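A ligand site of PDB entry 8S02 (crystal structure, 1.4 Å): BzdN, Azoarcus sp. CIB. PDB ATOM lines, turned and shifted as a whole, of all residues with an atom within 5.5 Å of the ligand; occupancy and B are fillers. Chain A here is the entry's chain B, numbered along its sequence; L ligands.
FE3 of the ligand is bound by SG of Cys 73 (2.2 Å).
SG of Cys 100 binds FE4 of the ligand (2.2 Å).
The side-chain sulfur of Cys 263 is bound to an iron atom (FE7) of the ligand, 2.3 Å away.
The side-chain sulfur of Cys 327 is bound to an iron atom (FE2) of the ligand, 2.3 Å away.
An iron atom (FE5) of the ligand is bound by the side-chain sulfur (SG) of Cys 36, 2.3 Å away.
The side-chain sulfur (SG) of Cys 293 binds an iron atom (FE6) of the ligand, 2.3 Å away.
S4 of the ligand sits close to OG of Ser 239 (3.2 Å).
S1 of the ligand sits close to OE1 of Gln 102 (3.6 Å).
A sulfur (S5) of the ligand sits close to a ring nitrogen (NE2) of His 330, at 3.5 Å.
A sulfur (S8) of the ligand lies close to the guanidinium group (NH2) of Arg 290 (3.5 Å).
S6 of the ligand lies close to NH2 of Arg 53, at 3.6 Å.
OG1 of Thr 37 lies close to S8 of the ligand (3.6 Å).
NH1 of Arg 267 lies close to S5 of the ligand.
The side-chain sulfur of Cys 100 lies close to the backbone NH of Gln 102.
The side-chain sulfur (SG) of Cys 263 sits close to the side-chain hydroxyl (OG1) of Thr 37, at 3.3 Å.
SG of Cys 36 lies close to N of Tyr 38.
The side-chain sulfur (SG) of Cys 293 sits close to the side-chain hydroxyl (OG) of Ser 99, at 3.2 Å.
The side-chain amide nitrogen (NE2) of Gln 102 lies within hydrogen-bond range of the backbone carbonyl oxygen (O) of Phe 326, 3.0 Å away.
The guanidinium group of Arg 290 lies within hydrogen-bond range of the side-chain hydroxyl of Thr 37, 2.7 Å away.
NH2 of Arg 53 sits at hydrogen-bond distance from OH of Tyr 103.
NH1 of Arg 53 lies within salt-bridge range of OE1 of Glu 240, 2.8 Å away.
Residues that only touch the ligand: Tyr 38, Phe 75, Ser 99, Tyr 103 and Gln 324.
Within 4 Å of the ligand: Cys 36, Thr 37, Tyr 38, Arg 53, Cys 73, Phe 75, Ser 99, Cys 100, Gln 102, Tyr 103, Ser 239, Cys 263, Arg 267, Arg 290, Cys 293, Gln 324, Cys 327 and His 330.
The nearest printed residue that does not touch the ligand is Pro 329 (4.05 Å).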
ATOM      1  N   CYS A  36     -15.461   5.763 -23.818  1.00  0.00           N
ATOM      2  CA  CYS A  36     -15.325   7.151 -24.245  1.00  0.00           C
ATOM      3  C   CYS A  36     -15.745   8.142 -23.163  1.00  0.00           C
ATOM      4  O   CYS A  36     -16.757   7.981 -22.454  1.00  0.00           O
ATOM      5  CB  CYS A  36     -16.027   7.423 -25.590  1.00  0.00           C
ATOM      6  SG  CYS A  36     -15.732   9.139 -26.193  1.00  0.00           S
ATOM      7  N   THR A  37     -14.969   9.191 -23.055  1.00  0.00           N
ATOM      8  CA  THR A  37     -15.217  10.197 -22.040  1.00  0.00           C
ATOM      9  C   THR A  37     -16.497  11.004 -22.274  1.00  0.00           C
ATOM     10  O   THR A  37     -16.833  11.826 -21.436  1.00  0.00           O
ATOM     11  CB  THR A  37     -14.007  11.126 -22.012  1.00  0.00           C
ATOM     12  OG1 THR A  37     -13.784  11.588 -23.351  1.00  0.00           O
ATOM     13  CG2 THR A  37     -12.772  10.362 -21.523  1.00  0.00           C
ATOM     14  N   TYR A  38     -17.211  10.793 -23.379  1.00  0.00           N
ATOM     15  CA  TYR A  38     -18.450  11.517 -23.627  1.00  0.00           C
ATOM     16  C   TYR A  38     -19.665  10.878 -22.943  1.00  0.00           C
ATOM     17  O   TYR A  38     -20.765  11.417 -23.039  1.00  0.00           O
ATOM     18  CB  TYR A  38     -18.699  11.640 -25.140  1.00  0.00           C
ATOM     19  CG  TYR A  38     -17.952  12.794 -25.792  1.00  0.00           C
ATOM     20  CD1 TYR A  38     -18.221  14.107 -25.445  1.00  0.00           C
ATOM     21  CD2 TYR A  38     -17.018  12.576 -26.810  1.00  0.00           C
ATOM     22  CE1 TYR A  38     -17.559  15.176 -26.031  1.00  0.00           C
ATOM     23  CE2 TYR A  38     -16.346  13.652 -27.424  1.00  0.00           C
ATOM     24  CZ  TYR A  38     -16.640  14.956 -27.058  1.00  0.00           C
ATOM     25  OH  TYR A  38     -15.969  15.993 -27.639  1.00  0.00           O
ATOM     26  N   ARG A  53     -14.857   3.568 -16.216  1.00  0.00           N
ATOM     27  CA  ARG A  53     -14.333   3.653 -17.571  1.00  0.00           C
ATOM     28  C   ARG A  53     -13.467   2.439 -17.893  1.00  0.00           C
ATOM     29  O   ARG A  53     -12.519   2.123 -17.186  1.00  0.00           O
ATOM     30  CB  ARG A  53     -13.520   4.941 -17.739  1.00  0.00           C
ATOM     31  CG  ARG A  53     -12.864   5.037 -19.110  1.00  0.00           C
ATOM     32  CD  ARG A  53     -13.245   6.304 -19.857  1.00  0.00           C
ATOM     33  NE  ARG A  53     -12.601   6.314 -21.166  1.00  0.00           N
ATOM     34  CZ  ARG A  53     -11.412   6.829 -21.444  1.00  0.00           C
ATOM     35  NH1 ARG A  53     -10.737   7.555 -20.570  1.00  0.00           N
ATOM     36  NH2 ARG A  53     -10.899   6.636 -22.663  1.00  0.00           N
ATOM     37  N   CYS A  73      -6.675   0.310 -33.599  1.00  0.00           N
ATOM     38  CA  CYS A  73      -5.699   0.822 -32.661  1.00  0.00           C
ATOM     39  C   CYS A  73      -5.503  -0.132 -31.479  1.00  0.00           C
ATOM     40  O   CYS A  73      -6.409  -0.916 -31.139  1.00  0.00           O
ATOM     41  CB  CYS A  73      -6.130   2.192 -32.149  1.00  0.00           C
ATOM     42  SG  CYS A  73      -7.574   2.148 -31.048  1.00  0.00           S
ATOM     43  N   PHE A  75      -5.539   0.578 -28.331  1.00  0.00           N
ATOM     44  CA  PHE A  75      -6.402   0.878 -27.203  1.00  0.00           C
ATOM     45  C   PHE A  75      -7.757   0.181 -27.329  1.00  0.00           C
ATOM     46  O   PHE A  75      -8.236  -0.402 -26.352  1.00  0.00           O
ATOM     47  CB  PHE A  75      -6.602   2.388 -27.077  1.00  0.00           C
ATOM     48  CG  PHE A  75      -7.507   2.808 -25.945  1.00  0.00           C
ATOM     49  CD1 PHE A  75      -7.267   2.377 -24.648  1.00  0.00           C
ATOM     50  CD2 PHE A  75      -8.541   3.689 -26.159  1.00  0.00           C
ATOM     51  CE1 PHE A  75      -8.091   2.790 -23.598  1.00  0.00           C
ATOM     52  CE2 PHE A  75      -9.358   4.096 -25.130  1.00  0.00           C
ATOM     53  CZ  PHE A  75      -9.134   3.653 -23.859  1.00  0.00           C
ATOM     54  N   CYS A  76      -8.375   0.215 -28.522  1.00  0.00           N
ATOM     55  CA  CYS A  76      -9.689  -0.427 -28.682  1.00  0.00           C
ATOM     56  C   CYS A  76      -9.600  -1.925 -28.485  1.00  0.00           C
ATOM     57  O   CYS A  76     -10.546  -2.548 -27.957  1.00  0.00           O
ATOM     58  CB  CYS A  76     -10.372  -0.019 -30.001  1.00  0.00           C
ATOM     59  SG  CYS A  76      -9.833  -0.861 -31.523  1.00  0.00           S
ATOM     60  N   SER A  99     -18.172   8.518 -30.564  1.00  0.00           N
ATOM     61  CA  SER A  99     -17.133   9.376 -31.140  1.00  0.00           C
ATOM     62  C   SER A  99     -16.383   8.532 -32.158  1.00  0.00           C
ATOM     63  O   SER A  99     -16.985   8.048 -33.117  1.00  0.00           O
ATOM     64  CB  SER A  99     -16.221   9.994 -30.061  1.00  0.00           C
ATOM     65  OG  SER A  99     -15.551  11.153 -30.561  1.00  0.00           O
ATOM     66  N   CYS A 100     -15.089   8.302 -31.929  1.00  0.00           N
ATOM     67  CA  CYS A 100     -14.274   7.539 -32.883  1.00  0.00           C
ATOM     68  C   CYS A 100     -14.920   6.222 -33.286  1.00  0.00           C
ATOM     69  O   CYS A 100     -15.394   5.457 -32.437  1.00  0.00           O
ATOM     70  CB  CYS A 100     -12.921   7.253 -32.213  1.00  0.00           C
ATOM     71  SG  CYS A 100     -11.856   6.157 -33.157  1.00  0.00           S
ATOM     72  N   GLN A 102     -13.545   3.505 -34.419  1.00  0.00           N
ATOM     73  CA  GLN A 102     -12.820   2.304 -34.000  1.00  0.00           C
ATOM     74  C   GLN A 102     -13.293   1.829 -32.636  1.00  0.00           C
ATOM     75  O   GLN A 102     -13.450   0.620 -32.412  1.00  0.00           O
ATOM     76  CB  GLN A 102     -11.312   2.600 -33.959  1.00  0.00           C
ATOM     77  CG  GLN A 102     -10.716   3.084 -35.303  1.00  0.00           C
ATOM     78  CD  GLN A 102      -9.240   2.800 -35.369  1.00  0.00           C
ATOM     79  OE1 GLN A 102      -8.726   1.984 -34.600  1.00  0.00           O
ATOM     80  NE2 GLN A 102      -8.535   3.484 -36.270  1.00  0.00           N
ATOM     81  N   TYR A 103     -13.515   2.768 -31.712  1.00  0.00           N
ATOM     82  CA  TYR A 103     -13.951   2.435 -30.362  1.00  0.00           C
ATOM     83  C   TYR A 103     -15.333   1.804 -30.372  1.00  0.00           C
ATOM     84  O   TYR A 103     -15.688   1.033 -29.471  1.00  0.00           O
ATOM     85  CB  TYR A 103     -14.001   3.766 -29.615  1.00  0.00           C
ATOM     86  CG  TYR A 103     -13.681   3.810 -28.144  1.00  0.00           C
ATOM     87  CD1 TYR A 103     -13.917   2.720 -27.301  1.00  0.00           C
ATOM     88  CD2 TYR A 103     -13.163   4.984 -27.592  1.00  0.00           C
ATOM     89  CE1 TYR A 103     -13.626   2.816 -25.926  1.00  0.00           C
ATOM     90  CE2 TYR A 103     -12.860   5.093 -26.260  1.00  0.00           C
ATOM     91  CZ  TYR A 103     -13.094   4.015 -25.424  1.00  0.00           C
ATOM     92  OH  TYR A 103     -12.789   4.170 -24.084  1.00  0.00           O
ATOM     93  N   GLY A 238      -2.530  13.497 -26.811  1.00  0.00           N
ATOM     94  CA  GLY A 238      -2.912  12.288 -27.502  1.00  0.00           C
ATOM     95  C   GLY A 238      -4.376  11.973 -27.272  1.00  0.00           C
ATOM     96  O   GLY A 238      -5.170  12.837 -26.895  1.00  0.00           O
ATOM     97  N   SER A 239      -4.710  10.725 -27.553  1.00  0.00           N
ATOM     98  CA  SER A 239      -6.088  10.289 -27.398  1.00  0.00           C
ATOM     99  C   SER A 239      -6.355   9.994 -25.932  1.00  0.00           C
ATOM    100  O   SER A 239      -6.883  10.842 -25.210  1.00  0.00           O
ATOM    101  CB  SER A 239      -6.367   9.081 -28.317  1.00  0.00           C
ATOM    102  OG  SER A 239      -5.497   7.999 -28.069  1.00  0.00           O
ATOM    103  N   GLU A 240      -5.961   8.807 -25.474  1.00  0.00           N
ATOM    104  CA  GLU A 240      -6.197   8.396 -24.095  1.00  0.00           C
ATOM    105  C   GLU A 240      -5.013   8.717 -23.179  1.00  0.00           C
ATOM    106  O   GLU A 240      -5.178   9.417 -22.170  1.00  0.00           O
ATOM    107  CB  GLU A 240      -6.583   6.912 -24.043  1.00  0.00           C
ATOM    108  CG  GLU A 240      -6.609   6.298 -22.634  1.00  0.00           C
ATOM    109  CD  GLU A 240      -7.519   7.022 -21.639  1.00  0.00           C
ATOM    110  OE1 GLU A 240      -8.398   7.815 -22.045  1.00  0.00           O
ATOM    111  OE2 GLU A 240      -7.355   6.780 -20.420  1.00  0.00           O
ATOM    112  N   CYS A 263      -7.545  12.264 -22.924  1.00  0.00           N
ATOM    113  CA  CYS A 263      -8.777  11.829 -22.240  1.00  0.00           C
ATOM    114  C   CYS A 263      -8.532  11.149 -20.883  1.00  0.00           C
ATOM    115  O   CYS A 263      -9.480  10.996 -20.091  1.00  0.00           O
ATOM    116  CB  CYS A 263      -9.638  11.014 -23.222  1.00  0.00           C
ATOM    117  SG  CYS A 263     -10.644  12.108 -24.204  1.00  0.00           S
ATOM    118  N   ARG A 267      -8.996  16.502 -21.242  1.00  0.00           N
ATOM    119  CA  ARG A 267     -10.112  16.484 -22.173  1.00  0.00           C
ATOM    120  C   ARG A 267     -11.326  15.803 -21.546  1.00  0.00           C
ATOM    121  O   ARG A 267     -12.452  16.000 -22.010  1.00  0.00           O
ATOM    122  CB  ARG A 267      -9.723  15.762 -23.475  1.00  0.00           C
ATOM    123  CG  ARG A 267     -10.616  16.153 -24.677  1.00  0.00           C
ATOM    124  CD  ARG A 267     -10.320  15.340 -25.943  1.00  0.00           C
ATOM    125  NE  ARG A 267      -8.987  15.620 -26.468  1.00  0.00           N
ATOM    126  CZ  ARG A 267      -8.016  14.731 -26.521  1.00  0.00           C
ATOM    127  NH1 ARG A 267      -8.182  13.493 -26.049  1.00  0.00           N
ATOM    128  NH2 ARG A 267      -6.831  15.079 -27.015  1.00  0.00           N
ATOM    129  N   ARG A 290     -17.641  20.847 -24.342  1.00  0.00           N
ATOM    130  CA  ARG A 290     -16.348  20.372 -23.848  1.00  0.00           C
ATOM    131  C   ARG A 290     -15.300  20.490 -24.961  1.00  0.00           C
ATOM    132  O   ARG A 290     -15.635  20.390 -26.146  1.00  0.00           O
ATOM    133  CB  ARG A 290     -16.500  18.885 -23.513  1.00  0.00           C
ATOM    134  CG  ARG A 290     -15.363  18.266 -22.695  1.00  0.00           C
ATOM    135  CD  ARG A 290     -15.348  16.741 -22.788  1.00  0.00           C
ATOM    136  NE  ARG A 290     -14.797  16.361 -24.088  1.00  0.00           N
ATOM    137  CZ  ARG A 290     -14.473  15.115 -24.386  1.00  0.00           C
ATOM    138  NH1 ARG A 290     -14.828  14.102 -23.613  1.00  0.00           N
ATOM    139  NH2 ARG A 290     -13.802  14.863 -25.504  1.00  0.00           N
ATOM    140  N   CYS A 293     -13.090  15.991 -28.972  1.00  0.00           N
ATOM    141  CA  CYS A 293     -12.361  14.928 -29.645  1.00  0.00           C
ATOM    142  C   CYS A 293     -12.080  15.370 -31.080  1.00  0.00           C
ATOM    143  O   CYS A 293     -12.927  16.034 -31.680  1.00  0.00           O
ATOM    144  CB  CYS A 293     -13.269  13.691 -29.740  1.00  0.00           C
ATOM    145  SG  CYS A 293     -12.527  12.243 -30.496  1.00  0.00           S
ATOM    146  N   PRO A 294     -10.915  15.022 -31.662  1.00  0.00           N
ATOM    147  CA  PRO A 294     -10.708  15.313 -33.098  1.00  0.00           C
ATOM    148  C   PRO A 294     -11.860  14.903 -33.999  1.00  0.00           C
ATOM    149  O   PRO A 294     -12.176  15.627 -34.950  1.00  0.00           O
ATOM    150  CB  PRO A 294      -9.413  14.547 -33.417  1.00  0.00           C
ATOM    151  CG  PRO A 294      -8.650  14.573 -32.108  1.00  0.00           C
ATOM    152  CD  PRO A 294      -9.705  14.443 -31.033  1.00  0.00           C
ATOM    153  N   GLN A 324      -1.368   6.467 -30.461  1.00  0.00           N
ATOM    154  CA  GLN A 324      -1.629   5.058 -30.633  1.00  0.00           C
ATOM    155  C   GLN A 324      -1.449   4.702 -32.104  1.00  0.00           C
ATOM    156  O   GLN A 324      -1.839   5.470 -32.993  1.00  0.00           O
ATOM    157  CB  GLN A 324      -3.053   4.730 -30.225  1.00  0.00           C
ATOM    158  CG  GLN A 324      -3.287   4.963 -28.727  1.00  0.00           C
ATOM    159  CD  GLN A 324      -2.678   3.878 -27.882  1.00  0.00           C
ATOM    160  OE1 GLN A 324      -3.081   2.718 -27.966  1.00  0.00           O
ATOM    161  NE2 GLN A 324      -1.696   4.254 -27.063  1.00  0.00           N
ATOM    162  N   PHE A 326      -2.260   3.492 -35.561  1.00  0.00           N
ATOM    163  CA  PHE A 326      -3.494   3.412 -36.355  1.00  0.00           C
ATOM    164  C   PHE A 326      -4.572   4.411 -35.954  1.00  0.00           C
ATOM    165  O   PHE A 326      -5.680   4.331 -36.458  1.00  0.00           O
ATOM    166  CB  PHE A 326      -4.090   1.983 -36.388  1.00  0.00           C
ATOM    167  CG  PHE A 326      -3.124   0.920 -36.827  1.00  0.00           C
ATOM    168  CD1 PHE A 326      -2.530   0.981 -38.069  1.00  0.00           C
ATOM    169  CD2 PHE A 326      -2.829  -0.149 -35.990  1.00  0.00           C
ATOM    170  CE1 PHE A 326      -1.637  -0.005 -38.488  1.00  0.00           C
ATOM    171  CE2 PHE A 326      -1.952  -1.144 -36.402  1.00  0.00           C
ATOM    172  CZ  PHE A 326      -1.351  -1.084 -37.656  1.00  0.00           C
ATOM    173  N   CYS A 327      -4.274   5.382 -35.075  1.00  0.00           N
ATOM    174  CA  CYS A 327      -5.308   6.297 -34.559  1.00  0.00           C
ATOM    175  C   CYS A 327      -5.686   7.345 -35.608  1.00  0.00           C
ATOM    176  O   CYS A 327      -5.078   8.416 -35.684  1.00  0.00           O
ATOM    177  CB  CYS A 327      -4.783   6.960 -33.293  1.00  0.00           C
ATOM    178  SG  CYS A 327      -5.952   8.082 -32.516  1.00  0.00           S
ATOM    179  N   ASP A 328      -6.750   7.074 -36.365  1.00  0.00           N
ATOM    180  CA  ASP A 328      -7.182   7.992 -37.428  1.00  0.00           C
ATOM    181  C   ASP A 328      -7.562   9.387 -36.969  1.00  0.00           C
ATOM    182  O   ASP A 328      -7.112  10.357 -37.621  1.00  0.00           O
ATOM    183  CB  ASP A 328      -8.318   7.357 -38.238  1.00  0.00           C
ATOM    184  CG  ASP A 328      -7.866   6.127 -38.958  1.00  0.00           C
ATOM    185  OD1 ASP A 328      -7.101   6.263 -39.933  1.00  0.00           O
ATOM    186  OD2 ASP A 328      -8.207   5.015 -38.509  1.00  0.00           O
ATOM    187  N   PRO A 329      -8.332   9.599 -35.914  1.00  0.00           N
ATOM    188  CA  PRO A 329      -8.742  10.993 -35.624  1.00  0.00           C
ATOM    189  C   PRO A 329      -7.545  11.846 -35.276  1.00  0.00           C
ATOM    190  O   PRO A 329      -7.436  12.984 -35.756  1.00  0.00           O
ATOM    191  CB  PRO A 329      -9.732  10.852 -34.457  1.00  0.00           C
ATOM    192  CG  PRO A 329     -10.247   9.442 -34.598  1.00  0.00           C
ATOM    193  CD  PRO A 329      -9.041   8.645 -35.032  1.00  0.00           C
ATOM    194  N   HIS A 330      -6.621  11.318 -34.471  1.00  0.00           N
ATOM    195  CA  HIS A 330      -5.473  12.117 -34.077  1.00  0.00           C
ATOM    196  C   HIS A 330      -4.437  12.177 -35.179  1.00  0.00           C
ATOM    197  O   HIS A 330      -3.699  13.176 -35.271  1.00  0.00           O
ATOM    198  CB  HIS A 330      -4.923  11.547 -32.771  1.00  0.00           C
ATOM    199  CG  HIS A 330      -5.843  11.749 -31.618  1.00  0.00           C
ATOM    200  ND1 HIS A 330      -5.658  12.770 -30.713  1.00  0.00           N
ATOM    201  CD2 HIS A 330      -6.980  11.115 -31.254  1.00  0.00           C
ATOM    202  CE1 HIS A 330      -6.631  12.730 -29.823  1.00  0.00           C
ATOM    203  NE2 HIS A 330      -7.460  11.742 -30.133  1.00  0.00           N
HETATM  204  S1  LIG L   1      -8.309   5.164 -32.989  1.00  0.00           S
HETATM  205  S2  LIG L   1     -10.310   4.574 -30.005  1.00  0.00           S
HETATM  206  S3  LIG L   1      -9.353   7.979 -30.934  1.00  0.00           S
HETATM  207  S4  LIG L   1      -6.905   5.642 -29.646  1.00  0.00           S
HETATM  208  S5  LIG L   1      -9.898  10.750 -27.821  1.00  0.00           S
HETATM  209  S6  LIG L   1     -11.876   8.813 -25.308  1.00  0.00           S
HETATM  210  S7  LIG L   1     -12.697   8.697 -28.809  1.00  0.00           S
HETATM  211  S8  LIG L   1     -13.243  11.696 -26.919  1.00  0.00           S
HETATM  212  S9  LIG L   1      -9.442   6.990 -27.189  1.00  0.00           S
HETATM  213 FE1  LIG L   1      -9.060   6.368 -29.296  1.00  0.00          FE
HETATM  214 FE2  LIG L   1      -7.533   6.749 -31.561  1.00  0.00          FE
HETATM  215 FE3  LIG L   1      -8.253   4.263 -30.882  1.00  0.00          FE
HETATM  216 FE4  LIG L   1     -10.064   5.995 -31.807  1.00  0.00          FE
HETATM  217 FE5  LIG L   1     -13.498   9.409 -26.779  1.00  0.00          FE
HETATM  218 FE6  LIG L   1     -12.003  10.888 -28.674  1.00  0.00          FE
HETATM  219 FE7  LIG L   1     -11.314  10.907 -26.019  1.00  0.00          FE
HETATM  220 FE8  LIG L   1     -10.911   8.691 -27.408  1.00  0.00          FE
